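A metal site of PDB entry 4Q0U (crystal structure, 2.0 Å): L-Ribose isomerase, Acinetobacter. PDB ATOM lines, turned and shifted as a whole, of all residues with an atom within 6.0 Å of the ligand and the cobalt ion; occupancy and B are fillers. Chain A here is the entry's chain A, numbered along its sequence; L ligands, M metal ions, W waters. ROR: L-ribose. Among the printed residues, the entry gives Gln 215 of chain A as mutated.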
ATOM      1  N   ILE A  51       5.946  22.011 -22.383  1.00  0.00           N
ATOM      2  CA  ILE A  51       5.952  22.779 -21.128  1.00  0.00           C
ATOM      3  C   ILE A  51       6.680  24.116 -21.226  1.00  0.00           C
ATOM      4  O   ILE A  51       7.771  24.219 -21.779  1.00  0.00           O
ATOM      5  CB  ILE A  51       6.600  21.938 -20.004  1.00  0.00           C
ATOM      6  CG1 ILE A  51       5.896  20.580 -19.913  1.00  0.00           C
ATOM      7  CG2 ILE A  51       6.501  22.667 -18.673  1.00  0.00           C
ATOM      8  CD1 ILE A  51       6.683  19.514 -19.176  1.00  0.00           C
ATOM      9  N   PHE A  53       7.783  27.026 -18.521  1.00  0.00           N
ATOM     10  CA  PHE A  53       7.879  27.297 -17.088  1.00  0.00           C
ATOM     11  C   PHE A  53       7.717  28.745 -16.632  1.00  0.00           C
ATOM     12  O   PHE A  53       8.678  29.390 -16.236  1.00  0.00           O
ATOM     13  CB  PHE A  53       9.206  26.742 -16.537  1.00  0.00           C
ATOM     14  CG  PHE A  53       9.401  25.275 -16.781  1.00  0.00           C
ATOM     15  CD1 PHE A  53      10.047  24.827 -17.933  1.00  0.00           C
ATOM     16  CD2 PHE A  53       8.952  24.333 -15.857  1.00  0.00           C
ATOM     17  CE1 PHE A  53      10.235  23.457 -18.161  1.00  0.00           C
ATOM     18  CE2 PHE A  53       9.137  22.962 -16.076  1.00  0.00           C
ATOM     19  CZ  PHE A  53       9.779  22.524 -17.228  1.00  0.00           C
ATOM     20  N   MET A  74      10.330  23.119 -22.396  1.00  0.00           N
ATOM     21  CA  MET A  74      10.746  21.808 -22.896  1.00  0.00           C
ATOM     22  C   MET A  74       9.565  20.911 -23.198  1.00  0.00           C
ATOM     23  O   MET A  74       8.415  21.219 -22.863  1.00  0.00           O
ATOM     24  CB  MET A  74      11.612  21.120 -21.844  1.00  0.00           C
ATOM     25  CG  MET A  74      10.786  20.603 -20.675  1.00  0.00           C
ATOM     26  SD  MET A  74      11.770  20.065 -19.276  1.00  0.00           S
ATOM     27  CE  MET A  74      12.530  18.574 -19.937  1.00  0.00           C
ATOM     28  N   ILE A  76       8.044  16.896 -22.946  1.00  0.00           N
ATOM     29  CA  ILE A  76       8.204  15.624 -22.278  1.00  0.00           C
ATOM     30  C   ILE A  76       7.115  14.645 -22.719  1.00  0.00           C
ATOM     31  O   ILE A  76       5.920  14.943 -22.632  1.00  0.00           O
ATOM     32  CB  ILE A  76       8.151  15.768 -20.735  1.00  0.00           C
ATOM     33  CG1 ILE A  76       9.320  16.643 -20.263  1.00  0.00           C
ATOM     34  CG2 ILE A  76       8.203  14.397 -20.078  1.00  0.00           C
ATOM     35  CD1 ILE A  76       9.360  16.878 -18.763  1.00  0.00           C
ATOM     36  N   LYS A 104      10.442   8.609 -19.591  1.00  0.00           N
ATOM     37  CA  LYS A 104      10.056   9.774 -20.372  1.00  0.00           C
ATOM     38  C   LYS A 104      11.132  10.143 -21.371  1.00  0.00           C
ATOM     39  O   LYS A 104      12.315   9.861 -21.150  1.00  0.00           O
ATOM     40  CB  LYS A 104       9.863  10.999 -19.466  1.00  0.00           C
ATOM     41  CG  LYS A 104       8.877  10.860 -18.336  1.00  0.00           C
ATOM     42  CD  LYS A 104       8.902  12.137 -17.479  1.00  0.00           C
ATOM     43  CE  LYS A 104       7.903  12.082 -16.335  1.00  0.00           C
ATOM     44  NZ  LYS A 104       8.008  13.298 -15.485  1.00  0.00           N
ATOM     45  N   MET A 106      12.730  13.421 -23.154  1.00  0.00           N
ATOM     46  CA  MET A 106      12.742  14.867 -22.997  1.00  0.00           C
ATOM     47  C   MET A 106      13.412  15.506 -24.203  1.00  0.00           C
ATOM     48  O   MET A 106      14.463  15.054 -24.665  1.00  0.00           O
ATOM     49  CB  MET A 106      13.488  15.281 -21.712  1.00  0.00           C
ATOM     50  CG  MET A 106      13.081  14.473 -20.469  1.00  0.00           C
ATOM     51  SD  MET A 106      13.846  15.074 -18.928  1.00  0.00           S
ATOM     52  CE  MET A 106      15.558  14.725 -19.250  1.00  0.00           C
ATOM     53  N   CYS A 114      15.659  23.198 -18.699  1.00  0.00           N
ATOM     54  CA  CYS A 114      14.707  22.527 -17.839  1.00  0.00           C
ATOM     55  C   CYS A 114      15.223  23.305 -16.609  1.00  0.00           C
ATOM     56  O   CYS A 114      16.403  23.184 -16.254  1.00  0.00           O
ATOM     57  CB  CYS A 114      15.015  21.043 -17.657  1.00  0.00           C
ATOM     58  SG  CYS A 114      13.980  20.313 -16.379  1.00  0.00           S
ATOM     59  N   PRO A 115      14.366  24.119 -15.972  1.00  0.00           N
ATOM     60  CA  PRO A 115      14.769  24.926 -14.807  1.00  0.00           C
ATOM     61  C   PRO A 115      15.171  24.282 -13.488  1.00  0.00           C
ATOM     62  O   PRO A 115      14.783  23.158 -13.171  1.00  0.00           O
ATOM     63  CB  PRO A 115      13.578  25.878 -14.648  1.00  0.00           C
ATOM     64  CG  PRO A 115      12.434  25.009 -15.010  1.00  0.00           C
ATOM     65  CD  PRO A 115      12.926  24.279 -16.251  1.00  0.00           C
ATOM     66  N   HIS A 117      15.440  22.860  -9.996  1.00  0.00           N
ATOM     67  CA  HIS A 117      14.430  22.273  -9.123  1.00  0.00           C
ATOM     68  C   HIS A 117      14.991  21.023  -8.483  1.00  0.00           C
ATOM     69  O   HIS A 117      16.074  20.546  -8.847  1.00  0.00           O
ATOM     70  CB  HIS A 117      13.166  21.909  -9.916  1.00  0.00           C
ATOM     71  CG  HIS A 117      13.367  20.764 -10.875  1.00  0.00           C
ATOM     72  ND1 HIS A 117      13.985  20.927 -12.099  1.00  0.00           N
ATOM     73  CD2 HIS A 117      13.065  19.451 -10.770  1.00  0.00           C
ATOM     74  CE1 HIS A 117      14.057  19.753 -12.699  1.00  0.00           C
ATOM     75  NE2 HIS A 117      13.503  18.843 -11.920  1.00  0.00           N
ATOM     76  N   HIS A 118      14.267  20.494  -7.498  1.00  0.00           N
ATOM     77  CA  HIS A 118      14.664  19.263  -6.843  1.00  0.00           C
ATOM     78  C   HIS A 118      13.400  18.517  -6.483  1.00  0.00           C
ATOM     79  O   HIS A 118      12.309  19.100  -6.463  1.00  0.00           O
ATOM     80  CB  HIS A 118      15.530  19.533  -5.603  1.00  0.00           C
ATOM     81  CG  HIS A 118      14.760  19.987  -4.387  1.00  0.00           C
ATOM     82  ND1 HIS A 118      14.381  21.294  -4.187  1.00  0.00           N
ATOM     83  CD2 HIS A 118      14.319  19.291  -3.318  1.00  0.00           C
ATOM     84  CE1 HIS A 118      13.743  21.387  -3.031  1.00  0.00           C
ATOM     85  NE2 HIS A 118      13.686  20.192  -2.478  1.00  0.00           N
ATOM     86  N   HIS A 119      13.524  17.222  -6.237  1.00  0.00           N
ATOM     87  CA  HIS A 119      12.383  16.393  -5.875  1.00  0.00           C
ATOM     88  C   HIS A 119      12.670  15.794  -4.518  1.00  0.00           C
ATOM     89  O   HIS A 119      13.802  15.378  -4.237  1.00  0.00           O
ATOM     90  CB  HIS A 119      12.224  15.255  -6.886  1.00  0.00           C
ATOM     91  CG  HIS A 119      12.154  15.714  -8.307  1.00  0.00           C
ATOM     92  ND1 HIS A 119      11.019  16.276  -8.855  1.00  0.00           N
ATOM     93  CD2 HIS A 119      13.090  15.734  -9.283  1.00  0.00           C
ATOM     94  CE1 HIS A 119      11.263  16.620 -10.110  1.00  0.00           C
ATOM     95  NE2 HIS A 119      12.507  16.306 -10.392  1.00  0.00           N
ATOM     96  N   LYS A 122      11.587  11.737  -5.846  1.00  0.00           N
ATOM     97  CA  LYS A 122      12.056  11.175  -7.109  1.00  0.00           C
ATOM     98  C   LYS A 122      13.552  11.243  -7.427  1.00  0.00           C
ATOM     99  O   LYS A 122      14.169  12.307  -7.367  1.00  0.00           O
ATOM    100  CB  LYS A 122      11.272  11.800  -8.261  1.00  0.00           C
ATOM    101  CG  LYS A 122      11.549  11.148  -9.627  1.00  0.00           C
ATOM    102  CD  LYS A 122      10.747  11.811 -10.738  1.00  0.00           C
ATOM    103  CE  LYS A 122      11.314  13.181 -11.077  1.00  0.00           C
ATOM    104  NZ  LYS A 122      10.600  13.820 -12.211  1.00  0.00           N
ATOM    105  N   GLU A 124      16.288  10.478 -10.437  1.00  0.00           N
ATOM    106  CA  GLU A 124      16.330  10.398 -11.895  1.00  0.00           C
ATOM    107  C   GLU A 124      17.641   9.850 -12.449  1.00  0.00           C
ATOM    108  O   GLU A 124      18.628   9.757 -11.734  1.00  0.00           O
ATOM    109  CB  GLU A 124      16.181  11.801 -12.510  1.00  0.00           C
ATOM    110  CG  GLU A 124      14.862  12.489 -12.318  1.00  0.00           C
ATOM    111  CD  GLU A 124      14.952  13.991 -12.592  1.00  0.00           C
ATOM    112  OE1 GLU A 124      15.814  14.405 -13.400  1.00  0.00           O
ATOM    113  OE2 GLU A 124      14.168  14.750 -11.993  1.00  0.00           O
ATOM    114  N   TYR A 126      19.800   9.919 -16.494  1.00  0.00           N
ATOM    115  CA  TYR A 126      19.765  10.455 -17.850  1.00  0.00           C
ATOM    116  C   TYR A 126      20.570   9.645 -18.859  1.00  0.00           C
ATOM    117  O   TYR A 126      21.679   9.184 -18.577  1.00  0.00           O
ATOM    118  CB  TYR A 126      20.308  11.891 -17.880  1.00  0.00           C
ATOM    119  CG  TYR A 126      19.802  12.788 -16.774  1.00  0.00           C
ATOM    120  CD1 TYR A 126      18.432  12.958 -16.563  1.00  0.00           C
ATOM    121  CD2 TYR A 126      20.691  13.480 -15.949  1.00  0.00           C
ATOM    122  CE1 TYR A 126      17.962  13.780 -15.536  1.00  0.00           C
ATOM    123  CE2 TYR A 126      20.233  14.308 -14.930  1.00  0.00           C
ATOM    124  CZ  TYR A 126      18.865  14.456 -14.730  1.00  0.00           C
ATOM    125  OH  TYR A 126      18.414  15.275 -13.720  1.00  0.00           O
ATOM    126  N   HIS A 199      18.824  20.470  -9.504  1.00  0.00           N
ATOM    127  CA  HIS A 199      19.342  20.210 -10.836  1.00  0.00           C
ATOM    128  C   HIS A 199      18.592  20.956 -11.918  1.00  0.00           C
ATOM    129  O   HIS A 199      17.437  21.356 -11.742  1.00  0.00           O
ATOM    130  CB  HIS A 199      19.325  18.699 -11.153  1.00  0.00           C
ATOM    131  CG  HIS A 199      17.969  18.064 -11.094  1.00  0.00           C
ATOM    132  ND1 HIS A 199      17.341  17.760  -9.904  1.00  0.00           N
ATOM    133  CD2 HIS A 199      17.120  17.667 -12.072  1.00  0.00           C
ATOM    134  CE1 HIS A 199      16.168  17.205 -10.156  1.00  0.00           C
ATOM    135  NE2 HIS A 199      16.010  17.143 -11.464  1.00  0.00           N
ATOM    136  N   PHE A 201      19.211  21.627 -16.581  1.00  0.00           N
ATOM    137  CA  PHE A 201      20.013  21.259 -17.732  1.00  0.00           C
ATOM    138  C   PHE A 201      19.557  22.013 -18.972  1.00  0.00           C
ATOM    139  O   PHE A 201      18.450  22.551 -19.021  1.00  0.00           O
ATOM    140  CB  PHE A 201      19.965  19.736 -17.954  1.00  0.00           C
ATOM    141  CG  PHE A 201      18.571  19.164 -18.084  1.00  0.00           C
ATOM    142  CD1 PHE A 201      17.923  19.139 -19.316  1.00  0.00           C
ATOM    143  CD2 PHE A 201      17.940  18.597 -16.987  1.00  0.00           C
ATOM    144  CE1 PHE A 201      16.647  18.559 -19.440  1.00  0.00           C
ATOM    145  CE2 PHE A 201      16.675  18.012 -17.099  1.00  0.00           C
ATOM    146  CZ  PHE A 201      16.027  17.987 -18.331  1.00  0.00           C
ATOM    147  N   GLN A 215      14.763   9.707 -19.907  1.00  0.00           N
ATOM    148  CA  GLN A 215      14.828   9.784 -18.456  1.00  0.00           C
ATOM    149  C   GLN A 215      14.157   8.574 -17.830  1.00  0.00           C
ATOM    150  O   GLN A 215      13.003   8.262 -18.142  1.00  0.00           O
ATOM    151  CB  GLN A 215      14.148  11.053 -17.927  1.00  0.00           C
ATOM    152  CG  GLN A 215      14.348  11.234 -16.405  1.00  0.00           C
ATOM    153  CD  GLN A 215      13.371  12.189 -15.764  1.00  0.00           C
ATOM    154  OE1 GLN A 215      13.147  13.290 -16.254  1.00  0.00           O
ATOM    155  NE2 GLN A 215      12.795  11.774 -14.642  1.00  0.00           N
ATOM    156  N   SER A 217      13.282   7.177 -14.127  1.00  0.00           N
ATOM    157  CA  SER A 217      13.265   7.603 -12.739  1.00  0.00           C
ATOM    158  C   SER A 217      12.209   6.855 -11.950  1.00  0.00           C
ATOM    159  O   SER A 217      11.495   6.015 -12.500  1.00  0.00           O
ATOM    160  CB  SER A 217      12.944   9.091 -12.666  1.00  0.00           C
ATOM    161  OG  SER A 217      11.566   9.305 -12.937  1.00  0.00           O
ATOM    162  N   SER A 220       6.675   9.589 -10.874  1.00  0.00           N
ATOM    163  CA  SER A 220       6.568  11.030 -11.033  1.00  0.00           C
ATOM    164  C   SER A 220       5.229  11.553 -10.499  1.00  0.00           C
ATOM    165  O   SER A 220       4.194  11.466 -11.167  1.00  0.00           O
ATOM    166  CB  SER A 220       6.739  11.384 -12.510  1.00  0.00           C
ATOM    167  OG  SER A 220       6.889  12.774 -12.707  1.00  0.00           O
ATOM    168  N   GLU A 222       2.840  14.174 -10.105  1.00  0.00           N
ATOM    169  CA  GLU A 222       2.572  15.483 -10.703  1.00  0.00           C
ATOM    170  C   GLU A 222       1.113  15.711 -11.043  1.00  0.00           C
ATOM    171  O   GLU A 222       0.638  15.308 -12.110  1.00  0.00           O
ATOM    172  CB  GLU A 222       3.410  15.655 -11.988  1.00  0.00           C
ATOM    173  CG  GLU A 222       4.916  15.456 -11.790  1.00  0.00           C
ATOM    174  CD  GLU A 222       5.703  15.681 -13.073  1.00  0.00           C
ATOM    175  OE1 GLU A 222       5.408  15.012 -14.088  1.00  0.00           O
ATOM    176  OE2 GLU A 222       6.629  16.528 -13.060  1.00  0.00           O
ATOM    177  N   ASN A 243       7.597  18.343  -7.014  1.00  0.00           N
ATOM    178  CA  ASN A 243       8.457  19.193  -7.829  1.00  0.00           C
ATOM    179  C   ASN A 243       8.641  20.555  -7.166  1.00  0.00           C
ATOM    180  O   ASN A 243       7.693  21.315  -7.027  1.00  0.00           O
ATOM    181  CB  ASN A 243       7.858  19.387  -9.229  1.00  0.00           C
ATOM    182  CG  ASN A 243       7.555  18.066  -9.917  1.00  0.00           C
ATOM    183  OD1 ASN A 243       8.371  17.144  -9.903  1.00  0.00           O
ATOM    184  ND2 ASN A 243       6.386  17.969 -10.544  1.00  0.00           N
ATOM    185  N   PHE A 245      10.537  23.967  -7.615  1.00  0.00           N
ATOM    186  CA  PHE A 245      11.334  24.862  -8.452  1.00  0.00           C
ATOM    187  C   PHE A 245      11.957  25.991  -7.643  1.00  0.00           C
ATOM    188  O   PHE A 245      11.303  26.590  -6.791  1.00  0.00           O
ATOM    189  CB  PHE A 245      10.450  25.439  -9.568  1.00  0.00           C
ATOM    190  CG  PHE A 245      10.097  24.437 -10.634  1.00  0.00           C
ATOM    191  CD1 PHE A 245      11.008  24.117 -11.642  1.00  0.00           C
ATOM    192  CD2 PHE A 245       8.884  23.761 -10.596  1.00  0.00           C
ATOM    193  CE1 PHE A 245      10.711  23.148 -12.589  1.00  0.00           C
ATOM    194  CE2 PHE A 245       8.576  22.786 -11.536  1.00  0.00           C
ATOM    195  CZ  PHE A 245       9.489  22.479 -12.532  1.00  0.00           C
ATOM    196  N   ARG A 254       3.912  25.406 -14.910  1.00  0.00           N
ATOM    197  CA  ARG A 254       4.487  24.075 -15.107  1.00  0.00           C
ATOM    198  C   ARG A 254       3.377  23.040 -15.279  1.00  0.00           C
ATOM    199  O   ARG A 254       3.548  22.045 -15.987  1.00  0.00           O
ATOM    200  CB  ARG A 254       5.372  23.704 -13.913  1.00  0.00           C
ATOM    201  CG  ARG A 254       6.351  22.552 -14.147  1.00  0.00           C
ATOM    202  CD  ARG A 254       5.663  21.212 -14.359  1.00  0.00           C
ATOM    203  NE  ARG A 254       6.621  20.148 -14.643  1.00  0.00           N
ATOM    204  CZ  ARG A 254       6.295  18.917 -15.030  1.00  0.00           C
ATOM    205  NH1 ARG A 254       7.235  18.015 -15.254  1.00  0.00           N
ATOM    206  NH2 ARG A 254       5.013  18.590 -15.187  1.00  0.00           N
HETATM  207  C5  ROR L   1      10.951  18.371 -15.305  1.00  0.00           C
HETATM  208  O5  ROR L   1      10.041  19.413 -15.032  1.00  0.00           O
HETATM  209  C4  ROR L   1      10.228  17.035 -15.226  1.00  0.00           C
HETATM  210  O4  ROR L   1       9.570  16.909 -13.967  1.00  0.00           O
HETATM  211  C3  ROR L   1      11.218  15.868 -15.428  1.00  0.00           C
HETATM  212  O3  ROR L   1      10.500  14.646 -15.370  1.00  0.00           O
HETATM  213  C2  ROR L   1      12.358  15.854 -14.404  1.00  0.00           C
HETATM  214  O2  ROR L   1      11.899  16.309 -13.147  1.00  0.00           O
HETATM  215  C1  ROR L   1      13.521  16.723 -14.881  1.00  0.00           C
HETATM  216  O1  ROR L   1      14.572  16.784 -14.222  1.00  0.00           O
HETATM  217 CO    CO M   1      13.794  16.632 -12.046  1.00  0.00          CO
HETATM  218  O   HOH W   1      10.354  11.978 -14.089  1.00  0.00           O
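The side-chain amino group (NZ) of Lys 104 is in hydrogen-bond range of an oxygen (O3) of the ligand, at 2.8 Å.
The side-chain carboxylate (OE2) of Glu 222 lies within hydrogen-bond range of an oxygen (O4) of the ligand, 3.1 Å away.
An oxygen (O3) of the ligand sits at hydrogen-bond distance from the side-chain amino group (NZ) of Lys 122 (3.3 Å).
The guanidinium group (NH1) of Arg 254 sits at hydrogen-bond distance from an oxygen (O4) of the ligand, 2.9 Å away.
O3 of the ligand lies within hydrogen-bond range of OE1 of Gln 215, 3.1 Å away.
NH1 of Arg 254 is in salt-bridge range of OE2 of Glu 222 (2.7 Å).
The side-chain carboxylate (OE1) of Glu 124 lies within hydrogen-bond range of the side-chain hydroxyl (OH) of Tyr 126 (2.8 Å).
OG of Ser 220 lies within hydrogen-bond range of NZ of Lys 104 (3.0 Å).
The side-chain carboxylate (OE2) of Glu 124 lies close to the side-chain amino group (NZ) of Lys 122 (3.7 Å).
SG of Cys 114 sits at hydrogen-bond distance from SD of Met 74 (3.7 Å).
A ring nitrogen (ND1) of His 119 lies close to the side-chain amide oxygen (OD1) of Asn 243 (3.0 Å).
OE2 of Glu 222 is in hydrogen-bond range of ND2 of Asn 243.
N of Gln 215 sits at hydrogen-bond distance from O of Lys 104 (2.7 Å).
The cobalt ion is bound by OE2 of Glu 124 (1.9 Å).
The cobalt ion is bound by NE2 of His 119 (2.1 Å).
An oxygen (O2) of the ligand is bound to the cobalt ion, 2.2 Å away.
NE2 of His 117 binds the cobalt ion, at 2.2 Å.
O1 of the ligand binds the cobalt ion (2.3 Å).
The cobalt ion is bound by NE2 of His 199 (2.3 Å).
Within 4 Å of the cobalt ion: His 117, His 119, Glu 124 and His 199.
Residues that only touch the ligand: Phe 53 (3.8 Å), Ile 76 (3.6 Å), Cys 114 (3.8 Å), Phe 201 (3.8 Å) and Phe 245 (3.99 Å).
Hydrophobic or aromatic side chains within 4 Å of the ligand: Phe 53, Ile 76, His 117, His 119, His 199, Phe 201 and Phe 245.
Along chain A the residues within 4 Å of the ligand span positions 53 to 254.
The nearest printed residue that does not touch the ligand is Tyr 126 (4.2 Å).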
